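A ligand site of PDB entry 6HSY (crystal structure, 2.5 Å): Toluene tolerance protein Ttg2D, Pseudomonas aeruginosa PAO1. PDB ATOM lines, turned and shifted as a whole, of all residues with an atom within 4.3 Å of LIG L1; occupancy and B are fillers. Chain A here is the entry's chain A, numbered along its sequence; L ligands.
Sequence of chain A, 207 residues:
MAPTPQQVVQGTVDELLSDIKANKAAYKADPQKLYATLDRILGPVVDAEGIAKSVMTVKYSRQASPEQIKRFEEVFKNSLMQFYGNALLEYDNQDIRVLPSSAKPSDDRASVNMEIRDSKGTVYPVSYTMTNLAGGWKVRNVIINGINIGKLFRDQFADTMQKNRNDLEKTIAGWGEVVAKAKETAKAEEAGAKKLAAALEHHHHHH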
ATOM      1  N   VAL A   9      -6.349  15.507  -0.974  1.00  0.00           N
ATOM      2  CA  VAL A   9      -5.445  16.289  -1.815  1.00  0.00           C
ATOM      3  C   VAL A   9      -6.155  16.688  -3.103  1.00  0.00           C
ATOM      4  O   VAL A   9      -6.241  17.872  -3.448  1.00  0.00           O
ATOM      5  CB  VAL A   9      -4.153  15.503  -2.096  1.00  0.00           C
ATOM      6  CG1 VAL A   9      -3.305  16.226  -3.143  1.00  0.00           C
ATOM      7  CG2 VAL A   9      -3.362  15.349  -0.826  1.00  0.00           C
ATOM      8  N   THR A  12      -8.766  19.263  -2.624  1.00  0.00           N
ATOM      9  CA  THR A  12      -8.223  20.586  -2.307  1.00  0.00           C
ATOM     10  C   THR A  12      -7.622  21.230  -3.540  1.00  0.00           C
ATOM     11  O   THR A  12      -7.778  22.443  -3.760  1.00  0.00           O
ATOM     12  CB  THR A  12      -7.196  20.473  -1.188  1.00  0.00           C
ATOM     13  OG1 THR A  12      -7.755  19.762  -0.076  1.00  0.00           O
ATOM     14  CG2 THR A  12      -6.756  21.859  -0.727  1.00  0.00           C
ATOM     15  N   VAL A  13      -6.915  20.457  -4.362  1.00  0.00           N
ATOM     16  CA  VAL A  13      -6.330  21.003  -5.586  1.00  0.00           C
ATOM     17  C   VAL A  13      -7.433  21.479  -6.521  1.00  0.00           C
ATOM     18  O   VAL A  13      -7.375  22.583  -7.075  1.00  0.00           O
ATOM     19  CB  VAL A  13      -5.433  19.949  -6.261  1.00  0.00           C
ATOM     20  CG1 VAL A  13      -4.855  20.493  -7.563  1.00  0.00           C
ATOM     21  CG2 VAL A  13      -4.301  19.541  -5.323  1.00  0.00           C
ATOM     22  N   LEU A  16      -9.286  24.638  -4.977  1.00  0.00           N
ATOM     23  CA  LEU A  16      -8.498  25.869  -4.959  1.00  0.00           C
ATOM     24  C   LEU A  16      -8.260  26.395  -6.362  1.00  0.00           C
ATOM     25  O   LEU A  16      -8.314  27.611  -6.599  1.00  0.00           O
ATOM     26  CB  LEU A  16      -7.176  25.629  -4.237  1.00  0.00           C
ATOM     27  CG  LEU A  16      -6.208  26.818  -4.170  1.00  0.00           C
ATOM     28  CD1 LEU A  16      -6.818  27.977  -3.388  1.00  0.00           C
ATOM     29  CD2 LEU A  16      -4.902  26.381  -3.547  1.00  0.00           C
ATOM     30  N   ASP A  39      -6.790  30.890   3.259  1.00  0.00           N
ATOM     31  CA  ASP A  39      -7.034  30.484   4.632  1.00  0.00           C
ATOM     32  C   ASP A  39      -8.301  29.647   4.749  1.00  0.00           C
ATOM     33  O   ASP A  39      -8.373  28.714   5.548  1.00  0.00           O
ATOM     34  CB  ASP A  39      -7.122  31.715   5.536  1.00  0.00           C
ATOM     35  CG  ASP A  39      -5.834  32.516   5.566  1.00  0.00           C
ATOM     36  OD1 ASP A  39      -4.745  31.910   5.395  1.00  0.00           O
ATOM     37  OD2 ASP A  39      -5.897  33.744   5.750  1.00  0.00           O
ATOM     38  N   LEU A  42      -7.304  26.127   2.467  1.00  0.00           N
ATOM     39  CA  LEU A  42      -6.173  25.349   2.964  1.00  0.00           C
ATOM     40  C   LEU A  42      -6.183  25.217   4.484  1.00  0.00           C
ATOM     41  O   LEU A  42      -5.676  24.225   5.017  1.00  0.00           O
ATOM     42  CB  LEU A  42      -4.863  25.979   2.507  1.00  0.00           C
ATOM     43  CG  LEU A  42      -4.659  26.071   0.993  1.00  0.00           C
ATOM     44  CD1 LEU A  42      -3.394  26.844   0.664  1.00  0.00           C
ATOM     45  CD2 LEU A  42      -4.618  24.691   0.364  1.00  0.00           C
ATOM     46  N   GLY A  43      -6.728  26.203   5.191  1.00  0.00           N
ATOM     47  CA  GLY A  43      -6.740  26.204   6.641  1.00  0.00           C
ATOM     48  C   GLY A  43      -7.140  24.872   7.240  1.00  0.00           C
ATOM     49  O   GLY A  43      -6.429  24.289   8.063  1.00  0.00           O
ATOM     50  N   VAL A  45      -7.083  21.950   6.123  1.00  0.00           N
ATOM     51  CA  VAL A  45      -6.298  20.797   5.712  1.00  0.00           C
ATOM     52  C   VAL A  45      -4.800  21.026   5.933  1.00  0.00           C
ATOM     53  O   VAL A  45      -3.967  20.357   5.324  1.00  0.00           O
ATOM     54  CB  VAL A  45      -6.587  20.420   4.247  1.00  0.00           C
ATOM     55  CG1 VAL A  45      -7.993  19.885   4.105  1.00  0.00           C
ATOM     56  CG2 VAL A  45      -6.367  21.612   3.331  1.00  0.00           C
ATOM     57  N   VAL A  46      -4.448  21.977   6.803  1.00  0.00           N
ATOM     58  CA  VAL A  46      -3.054  22.279   7.110  1.00  0.00           C
ATOM     59  C   VAL A  46      -2.857  22.144   8.615  1.00  0.00           C
ATOM     60  O   VAL A  46      -3.636  22.702   9.403  1.00  0.00           O
ATOM     61  CB  VAL A  46      -2.651  23.691   6.633  1.00  0.00           C
ATOM     62  CG1 VAL A  46      -1.316  24.119   7.238  1.00  0.00           C
ATOM     63  CG2 VAL A  46      -2.571  23.720   5.117  1.00  0.00           C
ATOM     64  N   ALA A  48      -0.918  23.566  10.885  1.00  0.00           N
ATOM     65  CA  ALA A  48      -0.044  24.711  11.121  1.00  0.00           C
ATOM     66  C   ALA A  48       0.761  24.527  12.404  1.00  0.00           C
ATOM     67  O   ALA A  48       1.985  24.753  12.424  1.00  0.00           O
ATOM     68  CB  ALA A  48      -0.855  25.995  11.180  1.00  0.00           C
ATOM     69  N   LYS A  77       2.786  31.839   8.189  1.00  0.00           N
ATOM     70  CA  LYS A  77       1.674  31.916   7.247  1.00  0.00           C
ATOM     71  C   LYS A  77       1.722  33.217   6.447  1.00  0.00           C
ATOM     72  O   LYS A  77       1.745  33.206   5.217  1.00  0.00           O
ATOM     73  CB  LYS A  77       0.340  31.820   7.998  1.00  0.00           C
ATOM     74  CG  LYS A  77       0.088  30.503   8.704  1.00  0.00           C
ATOM     75  CD  LYS A  77      -1.200  30.574   9.512  1.00  0.00           C
ATOM     76  CE  LYS A  77      -1.399  29.360  10.387  1.00  0.00           C
ATOM     77  NZ  LYS A  77      -2.689  29.400  11.126  1.00  0.00           N
ATOM     78  N   LEU A  80       4.556  33.508   3.999  1.00  0.00           N
ATOM     79  CA  LEU A  80       4.371  32.601   2.867  1.00  0.00           C
ATOM     80  C   LEU A  80       3.392  33.174   1.855  1.00  0.00           C
ATOM     81  O   LEU A  80       3.619  33.080   0.647  1.00  0.00           O
ATOM     82  CB  LEU A  80       3.893  31.231   3.363  1.00  0.00           C
ATOM     83  CG  LEU A  80       4.961  30.289   3.920  1.00  0.00           C
ATOM     84  CD1 LEU A  80       4.329  29.092   4.603  1.00  0.00           C
ATOM     85  CD2 LEU A  80       5.892  29.831   2.810  1.00  0.00           C
ATOM     86  N   MET A  81       2.298  33.778   2.331  1.00  0.00           N
ATOM     87  CA  MET A  81       1.321  34.365   1.415  1.00  0.00           C
ATOM     88  C   MET A  81       1.860  35.648   0.794  1.00  0.00           C
ATOM     89  O   MET A  81       1.599  35.931  -0.391  1.00  0.00           O
ATOM     90  CB  MET A  81       0.011  34.638   2.148  1.00  0.00           C
ATOM     91  CG  MET A  81      -0.647  33.386   2.726  1.00  0.00           C
ATOM     92  SD  MET A  81      -2.271  33.697   3.464  1.00  0.00           S
ATOM     93  CE  MET A  81      -1.853  34.854   4.766  1.00  0.00           C
ATOM     94  N   TYR A  84       4.777  34.405  -1.705  1.00  0.00           N
ATOM     95  CA  TYR A  84       4.501  33.303  -2.607  1.00  0.00           C
ATOM     96  C   TYR A  84       3.023  33.143  -2.927  1.00  0.00           C
ATOM     97  O   TYR A  84       2.641  32.133  -3.535  1.00  0.00           O
ATOM     98  CB  TYR A  84       5.057  31.991  -2.035  1.00  0.00           C
ATOM     99  CG  TYR A  84       6.540  32.046  -1.713  1.00  0.00           C
ATOM    100  CD1 TYR A  84       7.490  31.979  -2.719  1.00  0.00           C
ATOM    101  CD2 TYR A  84       6.983  32.162  -0.402  1.00  0.00           C
ATOM    102  CE1 TYR A  84       8.836  32.017  -2.439  1.00  0.00           C
ATOM    103  CE2 TYR A  84       8.335  32.202  -0.106  1.00  0.00           C
ATOM    104  CZ  TYR A  84       9.260  32.136  -1.135  1.00  0.00           C
ATOM    105  OH  TYR A  84      10.606  32.182  -0.850  1.00  0.00           O
ATOM    106  N   ALA A  87       2.074  33.594  -6.811  1.00  0.00           N
ATOM    107  CA  ALA A  87       2.458  32.491  -7.689  1.00  0.00           C
ATOM    108  C   ALA A  87       1.255  31.669  -8.116  1.00  0.00           C
ATOM    109  O   ALA A  87       1.252  31.095  -9.210  1.00  0.00           O
ATOM    110  CB  ALA A  87       3.487  31.604  -6.991  1.00  0.00           C
ATOM    111  N   LEU A  88       0.221  31.591  -7.268  1.00  0.00           N
ATOM    112  CA  LEU A  88      -0.958  30.794  -7.596  1.00  0.00           C
ATOM    113  C   LEU A  88      -1.819  31.445  -8.674  1.00  0.00           C
ATOM    114  O   LEU A  88      -2.649  30.763  -9.271  1.00  0.00           O
ATOM    115  CB  LEU A  88      -1.787  30.561  -6.337  1.00  0.00           C
ATOM    116  CG  LEU A  88      -1.114  29.739  -5.240  1.00  0.00           C
ATOM    117  CD1 LEU A  88      -1.931  29.788  -3.969  1.00  0.00           C
ATOM    118  CD2 LEU A  88      -0.907  28.299  -5.688  1.00  0.00           C
ATOM    119  N   TYR A  91       0.347  31.330 -12.772  1.00  0.00           N
ATOM    120  CA  TYR A  91       0.400  30.045 -13.463  1.00  0.00           C
ATOM    121  C   TYR A  91      -0.607  29.070 -12.840  1.00  0.00           C
ATOM    122  O   TYR A  91      -0.268  28.000 -12.348  1.00  0.00           O
ATOM    123  CB  TYR A  91       1.820  29.483 -13.460  1.00  0.00           C
ATOM    124  CG  TYR A  91       2.740  30.159 -14.457  1.00  0.00           C
ATOM    125  CD1 TYR A  91       2.270  30.529 -15.712  1.00  0.00           C
ATOM    126  CD2 TYR A  91       4.068  30.445 -14.148  1.00  0.00           C
ATOM    127  CE1 TYR A  91       3.081  31.151 -16.626  1.00  0.00           C
ATOM    128  CE2 TYR A  91       4.891  31.070 -15.067  1.00  0.00           C
ATOM    129  CZ  TYR A  91       4.394  31.420 -16.309  1.00  0.00           C
ATOM    130  OH  TYR A  91       5.205  32.042 -17.222  1.00  0.00           O
ATOM    131  N   ILE A  96      -1.936  19.466 -13.064  1.00  0.00           N
ATOM    132  CA  ILE A  96      -1.468  18.746 -11.882  1.00  0.00           C
ATOM    133  C   ILE A  96      -2.038  17.345 -11.923  1.00  0.00           C
ATOM    134  O   ILE A  96      -3.181  17.142 -12.340  1.00  0.00           O
ATOM    135  CB  ILE A  96      -1.864  19.468 -10.580  1.00  0.00           C
ATOM    136  CG1 ILE A  96      -1.221  20.862 -10.537  1.00  0.00           C
ATOM    137  CG2 ILE A  96      -1.446  18.650  -9.352  1.00  0.00           C
ATOM    138  CD1 ILE A  96      -1.606  21.696  -9.350  1.00  0.00           C
ATOM    139  N   ILE A 116       3.589  18.447 -11.498  1.00  0.00           N
ATOM    140  CA  ILE A 116       3.122  19.735 -11.998  1.00  0.00           C
ATOM    141  C   ILE A 116       3.770  19.946 -13.358  1.00  0.00           C
ATOM    142  O   ILE A 116       4.988  20.186 -13.443  1.00  0.00           O
ATOM    143  CB  ILE A 116       3.452  20.889 -11.043  1.00  0.00           C
ATOM    144  CG1 ILE A 116       2.783  20.658  -9.691  1.00  0.00           C
ATOM    145  CG2 ILE A 116       3.017  22.219 -11.654  1.00  0.00           C
ATOM    146  CD1 ILE A 116       3.084  21.727  -8.650  1.00  0.00           C
ATOM    147  N   TYR A 128       3.190  15.601  -0.562  1.00  0.00           N
ATOM    148  CA  TYR A 128       2.552  16.100   0.644  1.00  0.00           C
ATOM    149  C   TYR A 128       2.546  14.996   1.688  1.00  0.00           C
ATOM    150  O   TYR A 128       2.002  13.920   1.443  1.00  0.00           O
ATOM    151  CB  TYR A 128       1.121  16.574   0.349  1.00  0.00           C
ATOM    152  CG  TYR A 128       1.043  17.698  -0.657  1.00  0.00           C
ATOM    153  CD1 TYR A 128       1.126  17.429  -2.015  1.00  0.00           C
ATOM    154  CD2 TYR A 128       0.899  19.017  -0.254  1.00  0.00           C
ATOM    155  CE1 TYR A 128       1.051  18.452  -2.944  1.00  0.00           C
ATOM    156  CE2 TYR A 128       0.820  20.043  -1.170  1.00  0.00           C
ATOM    157  CZ  TYR A 128       0.906  19.755  -2.514  1.00  0.00           C
ATOM    158  OH  TYR A 128       0.832  20.769  -3.447  1.00  0.00           O
ATOM    159  N   MET A 130       0.977  13.620   4.777  1.00  0.00           N
ATOM    160  CA  MET A 130      -0.298  13.768   5.451  1.00  0.00           C
ATOM    161  C   MET A 130      -0.295  13.040   6.784  1.00  0.00           C
ATOM    162  O   MET A 130       0.375  12.014   6.968  1.00  0.00           O
ATOM    163  CB  MET A 130      -1.435  13.231   4.591  1.00  0.00           C
ATOM    164  CG  MET A 130      -1.636  13.977   3.287  1.00  0.00           C
ATOM    165  SD  MET A 130      -1.792  15.750   3.559  1.00  0.00           S
ATOM    166  CE  MET A 130      -2.361  16.276   1.960  1.00  0.00           C
ATOM    167  N   VAL A 139      -1.967  18.475   5.917  1.00  0.00           N
ATOM    168  CA  VAL A 139      -0.584  18.555   5.460  1.00  0.00           C
ATOM    169  C   VAL A 139       0.328  18.796   6.656  1.00  0.00           C
ATOM    170  O   VAL A 139       0.067  19.669   7.486  1.00  0.00           O
ATOM    171  CB  VAL A 139      -0.415  19.652   4.404  1.00  0.00           C
ATOM    172  CG1 VAL A 139       1.038  19.776   3.978  1.00  0.00           C
ATOM    173  CG2 VAL A 139      -1.284  19.376   3.193  1.00  0.00           C
ATOM    174  N   LYS A 183      13.175  30.535  -1.302  1.00  0.00           N
ATOM    175  CA  LYS A 183      13.208  30.071  -2.686  1.00  0.00           C
ATOM    176  C   LYS A 183      14.630  29.980  -3.203  1.00  0.00           C
ATOM    177  O   LYS A 183      15.061  28.921  -3.691  1.00  0.00           O
ATOM    178  CB  LYS A 183      12.367  31.005  -3.550  1.00  0.00           C
ATOM    179  CG  LYS A 183      12.155  30.558  -4.987  1.00  0.00           C
ATOM    180  CD  LYS A 183      11.942  31.786  -5.863  1.00  0.00           C
ATOM    181  CE  LYS A 183      11.206  31.473  -7.140  1.00  0.00           C
ATOM    182  NZ  LYS A 183      11.235  32.679  -8.016  1.00  0.00           N
ATOM    183  N   LYS A 187      17.075  26.931  -4.402  1.00  0.00           N
ATOM    184  CA  LYS A 187      17.784  26.876  -5.672  1.00  0.00           C
ATOM    185  C   LYS A 187      19.269  26.602  -5.459  1.00  0.00           C
ATOM    186  O   LYS A 187      19.843  25.701  -6.090  1.00  0.00           O
ATOM    187  CB  LYS A 187      17.599  28.182  -6.441  1.00  0.00           C
ATOM    188  CG  LYS A 187      16.161  28.482  -6.817  1.00  0.00           C
ATOM    189  CD  LYS A 187      15.620  27.467  -7.814  1.00  0.00           C
ATOM    190  CE  LYS A 187      14.201  27.805  -8.233  1.00  0.00           C
ATOM    191  NZ  LYS A 187      14.116  29.150  -8.839  1.00  0.00           N
HETATM  192  C1  LIG L   1       2.202  28.653  -2.450  1.00  0.00           C
HETATM  193  C2  LIG L   1       2.035  29.449  -1.134  1.00  0.00           C
HETATM  194  C3  LIG L   1       0.808  29.057  -0.280  1.00  0.00           C
HETATM  195  C4  LIG L   1       7.556  28.932  -9.001  1.00  0.00           C
HETATM  196  C5  LIG L   1       7.259  30.373  -8.342  1.00  0.00           C
HETATM  197  C6  LIG L   1       7.417  29.410  -6.098  1.00  0.00           C
HETATM  198  C7  LIG L   1       6.175  29.591  -5.157  1.00  0.00           C
HETATM  199  C8  LIG L   1       5.403  28.255  -4.848  1.00  0.00           C
HETATM  200  C9  LIG L   1       3.933  28.443  -4.404  1.00  0.00           C
HETATM  201  C10 LIG L   1       3.653  28.354  -2.882  1.00  0.00           C
HETATM  202  C11 LIG L   1       0.645  29.825   1.045  1.00  0.00           C
HETATM  203  C12 LIG L   1       0.230  28.985   2.276  1.00  0.00           C
HETATM  204  C13 LIG L   1      -0.798  29.663   3.193  1.00  0.00           C
HETATM  205  C14 LIG L   1      -1.204  28.839   4.436  1.00  0.00           C
HETATM  206  C15 LIG L   1      -2.709  28.848   4.786  1.00  0.00           C
HETATM  207  C16 LIG L   1      -3.128  27.832   5.860  1.00  0.00           C
HETATM  208  C17 LIG L   1      -3.599  28.434   7.183  1.00  0.00           C
HETATM  209  C18 LIG L   1      -3.518  27.489   8.382  1.00  0.00           C
HETATM  210  C19 LIG L   1       9.113  28.707  -9.111  1.00  0.00           C
HETATM  211  C20 LIG L   1      11.512  30.603 -10.835  1.00  0.00           C
HETATM  212  C21 LIG L   1      12.269  31.697 -11.651  1.00  0.00           C
HETATM  213  C22 LIG L   1      13.714  31.281 -12.081  1.00  0.00           C
HETATM  214  C23 LIG L   1       5.612  28.771 -10.413  1.00  0.00           C
HETATM  215  C24 LIG L   1       4.913  27.387 -10.152  1.00  0.00           C
HETATM  216  C25 LIG L   1       3.555  27.511  -9.366  1.00  0.00           C
HETATM  217  C26 LIG L   1       2.668  26.233  -9.329  1.00  0.00           C
HETATM  218  C27 LIG L   1       2.011  25.909  -7.954  1.00  0.00           C
HETATM  219  C28 LIG L   1       0.567  25.339  -7.998  1.00  0.00           C
HETATM  220  C29 LIG L   1       0.391  23.887  -7.451  1.00  0.00           C
HETATM  221  C30 LIG L   1      -0.960  23.603  -6.757  1.00  0.00           C
HETATM  222  C31 LIG L   1      -1.365  24.573  -5.645  1.00  0.00           C
HETATM  223  C32 LIG L   1      -0.516  24.656  -4.421  1.00  0.00           C
HETATM  224  C33 LIG L   1      -1.892  24.117  -4.270  1.00  0.00           C
HETATM  225  C34 LIG L   1      -2.084  22.648  -3.876  1.00  0.00           C
HETATM  226  C35 LIG L   1      -2.063  22.370  -2.380  1.00  0.00           C
HETATM  227  C36 LIG L   1      -2.797  21.120  -1.894  1.00  0.00           C
HETATM  228  C37 LIG L   1      -2.682  20.919  -0.363  1.00  0.00           C
HETATM  229  C38 LIG L   1      -2.927  19.488   0.143  1.00  0.00           C
HETATM  230  C39 LIG L   1      -4.047  19.399   1.183  1.00  0.00           C
HETATM  231  O1  LIG L   1       7.741  30.474  -6.962  1.00  0.00           O
HETATM  232  O2  LIG L   1       8.077  28.417  -6.095  1.00  0.00           O
HETATM  233  O3  LIG L   1       9.435  27.781 -10.083  1.00  0.00           O
HETATM  234  O4  LIG L   1       9.663  27.780 -12.703  1.00  0.00           O
HETATM  235  O5  LIG L   1      11.792  27.681 -11.184  1.00  0.00           O
HETATM  236  O6  LIG L   1      10.540  29.965 -11.564  1.00  0.00           O
HETATM  237  O7  LIG L   1      12.394  32.813 -10.827  1.00  0.00           O
HETATM  238  O8  LIG L   1      14.234  32.288 -12.886  1.00  0.00           O
HETATM  239  O9  LIG L   1       7.006  28.834 -10.333  1.00  0.00           O
HETATM  240  O10 LIG L   1       5.014  29.758 -10.640  1.00  0.00           O
HETATM  241  P1  LIG L   1      10.426  28.203 -11.497  1.00  0.00           P
HETATM  242  C1  LG2 L   2       3.126  23.728  -3.290  1.00  0.00           C
HETATM  243  C2  LG2 L   2       2.372  24.509  -2.163  1.00  0.00           C
HETATM  244  C3  LG2 L   2       1.725  23.640  -1.045  1.00  0.00           C
HETATM  245  C4  LG2 L   2      11.250  25.220  -8.723  1.00  0.00           C
HETATM  246  C5  LG2 L   2       9.798  24.551  -8.655  1.00  0.00           C
HETATM  247  C6  LG2 L   2       7.491  25.002  -8.041  1.00  0.00           C
HETATM  248  C7  LG2 L   2       6.829  25.075  -6.617  1.00  0.00           C
HETATM  249  C8  LG2 L   2       5.284  24.714  -6.591  1.00  0.00           C
HETATM  250  C9  LG2 L   2       4.792  23.903  -5.338  1.00  0.00           C
HETATM  251  C10 LG2 L   2       3.747  24.614  -4.420  1.00  0.00           C
HETATM  252  C11 LG2 L   2       0.971  24.420   0.082  1.00  0.00           C
HETATM  253  C12 LG2 L   2       0.754  23.684   1.431  1.00  0.00           C
HETATM  254  C13 LG2 L   2       0.282  24.606   2.598  1.00  0.00           C
HETATM  255  C14 LG2 L   2       1.195  24.625   3.860  1.00  0.00           C
HETATM  256  C15 LG2 L   2       1.042  25.881   4.776  1.00  0.00           C
HETATM  257  C16 LG2 L   2       2.068  25.991   5.929  1.00  0.00           C
HETATM  258  C17 LG2 L   2       1.693  26.987   7.056  1.00  0.00           C
HETATM  259  C18 LG2 L   2       2.688  27.046   8.215  1.00  0.00           C
HETATM  260  C19 LG2 L   2      12.377  24.126  -8.440  1.00  0.00           C
HETATM  261  C20 LG2 L   2      14.308  23.925 -13.277  1.00  0.00           C
HETATM  262  C21 LG2 L   2      15.398  23.136 -14.075  1.00  0.00           C
HETATM  263  C22 LG2 L   2      16.173  23.991 -15.136  1.00  0.00           C
HETATM  264  C23 LG2 L   2      11.683  25.931  -6.397  1.00  0.00           C
HETATM  265  C24 LG2 L   2      10.501  25.642  -5.414  1.00  0.00           C
HETATM  266  C25 LG2 L   2      10.863  25.881  -3.902  1.00  0.00           C
HETATM  267  C26 LG2 L   2      10.544  27.286  -3.323  1.00  0.00           C
HETATM  268  C27 LG2 L   2      10.519  27.374  -1.765  1.00  0.00           C
HETATM  269  C28 LG2 L   2       9.295  28.101  -1.133  1.00  0.00           C
HETATM  270  C29 LG2 L   2       8.388  27.224  -0.226  1.00  0.00           C
HETATM  271  C30 LG2 L   2       6.933  27.714  -0.089  1.00  0.00           C
HETATM  272  C31 LG2 L   2       5.791  26.750  -0.403  1.00  0.00           C
HETATM  273  C32 LG2 L   2       4.477  26.928   0.273  1.00  0.00           C
HETATM  274  C33 LG2 L   2       5.270  25.721   0.623  1.00  0.00           C
HETATM  275  C34 LG2 L   2       5.873  25.569   2.014  1.00  0.00           C
HETATM  276  C35 LG2 L   2       4.923  25.235   3.176  1.00  0.00           C
HETATM  277  C36 LG2 L   2       5.603  25.071   4.555  1.00  0.00           C
HETATM  278  C37 LG2 L   2       6.573  23.873   4.662  1.00  0.00           C
HETATM  279  C38 LG2 L   2       6.997  23.517   6.092  1.00  0.00           C
HETATM  280  C39 LG2 L   2       6.884  22.025   6.431  1.00  0.00           C
HETATM  281  O1  LG2 L   2       8.795  25.483  -8.158  1.00  0.00           O
HETATM  282  O2  LG2 L   2       6.933  24.544  -8.986  1.00  0.00           O
HETATM  283  O3  LG2 L   2      12.746  23.480  -9.596  1.00  0.00           O
HETATM  284  O4  LG2 L   2      15.288  23.942  -9.967  1.00  0.00           O
HETATM  285  O5  LG2 L   2      13.484  25.567 -10.940  1.00  0.00           O
HETATM  286  O6  LG2 L   2      13.963  23.286 -12.109  1.00  0.00           O
HETATM  287  O7  LG2 L   2      16.354  22.717 -13.153  1.00  0.00           O
HETATM  288  O8  LG2 L   2      17.311  23.278 -15.498  1.00  0.00           O
HETATM  289  O9  LG2 L   2      11.375  26.294  -7.726  1.00  0.00           O
HETATM  290  O10 LG2 L   2      12.819  25.853  -6.075  1.00  0.00           O
HETATM  291  P1  LG2 L   2      13.976  24.196 -10.614  1.00  0.00           P
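O5 of LIG L1 sits close to O5 of LG2 L2.
N of Val 139 is in hydrogen-bond range of O of Val 45, at 2.8 Å. The backbone NH (N) of Lys 183 sits at hydrogen-bond distance from the side-chain hydroxyl (OH) of Tyr 84 (3.1 Å). The backbone NH (N) of Val 139 lies close to the side-chain sulfur (SD) of Met 130 (3.6 Å).
An oxygen (O7) of LIG L1 lies within hydrogen-bond range of the side-chain amino group of Lys 183 (3.0 Å). The side-chain amino group of Lys 187 is in salt-bridge range of an oxygen (O5) of LIG L1.
Residues that only touch LIG L1: Thr 12 (3.9 Å), Leu 16 (3.8 Å), Asp 39 (3.7 Å), Gly 43 (3.9 Å), Val 45 (3.9 Å), Lys 77 (3.4 Å), Met 81 (3.8 Å), Tyr 84 (3.7 Å), Ala 87 (3.8 Å), Leu 88 (3.8 Å), Tyr 91 (3.7 Å), Ile 96 (3.3 Å), Ile 116 (3.7 Å), Tyr 128 (3.5 Å), Met 130 (3.6 Å) and Val 139 (3.4 Å). Hydrophobic or aromatic side chains that line LIG L1: Leu 16, Val 45, Met 81, Tyr 84, Ala 87, Leu 88, Tyr 91, Ile 96, Ile 116, Tyr 128, Met 130 and Val 139. The nearest printed residue that does not touch LIG L1 is Val 13 (4.1 Å).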
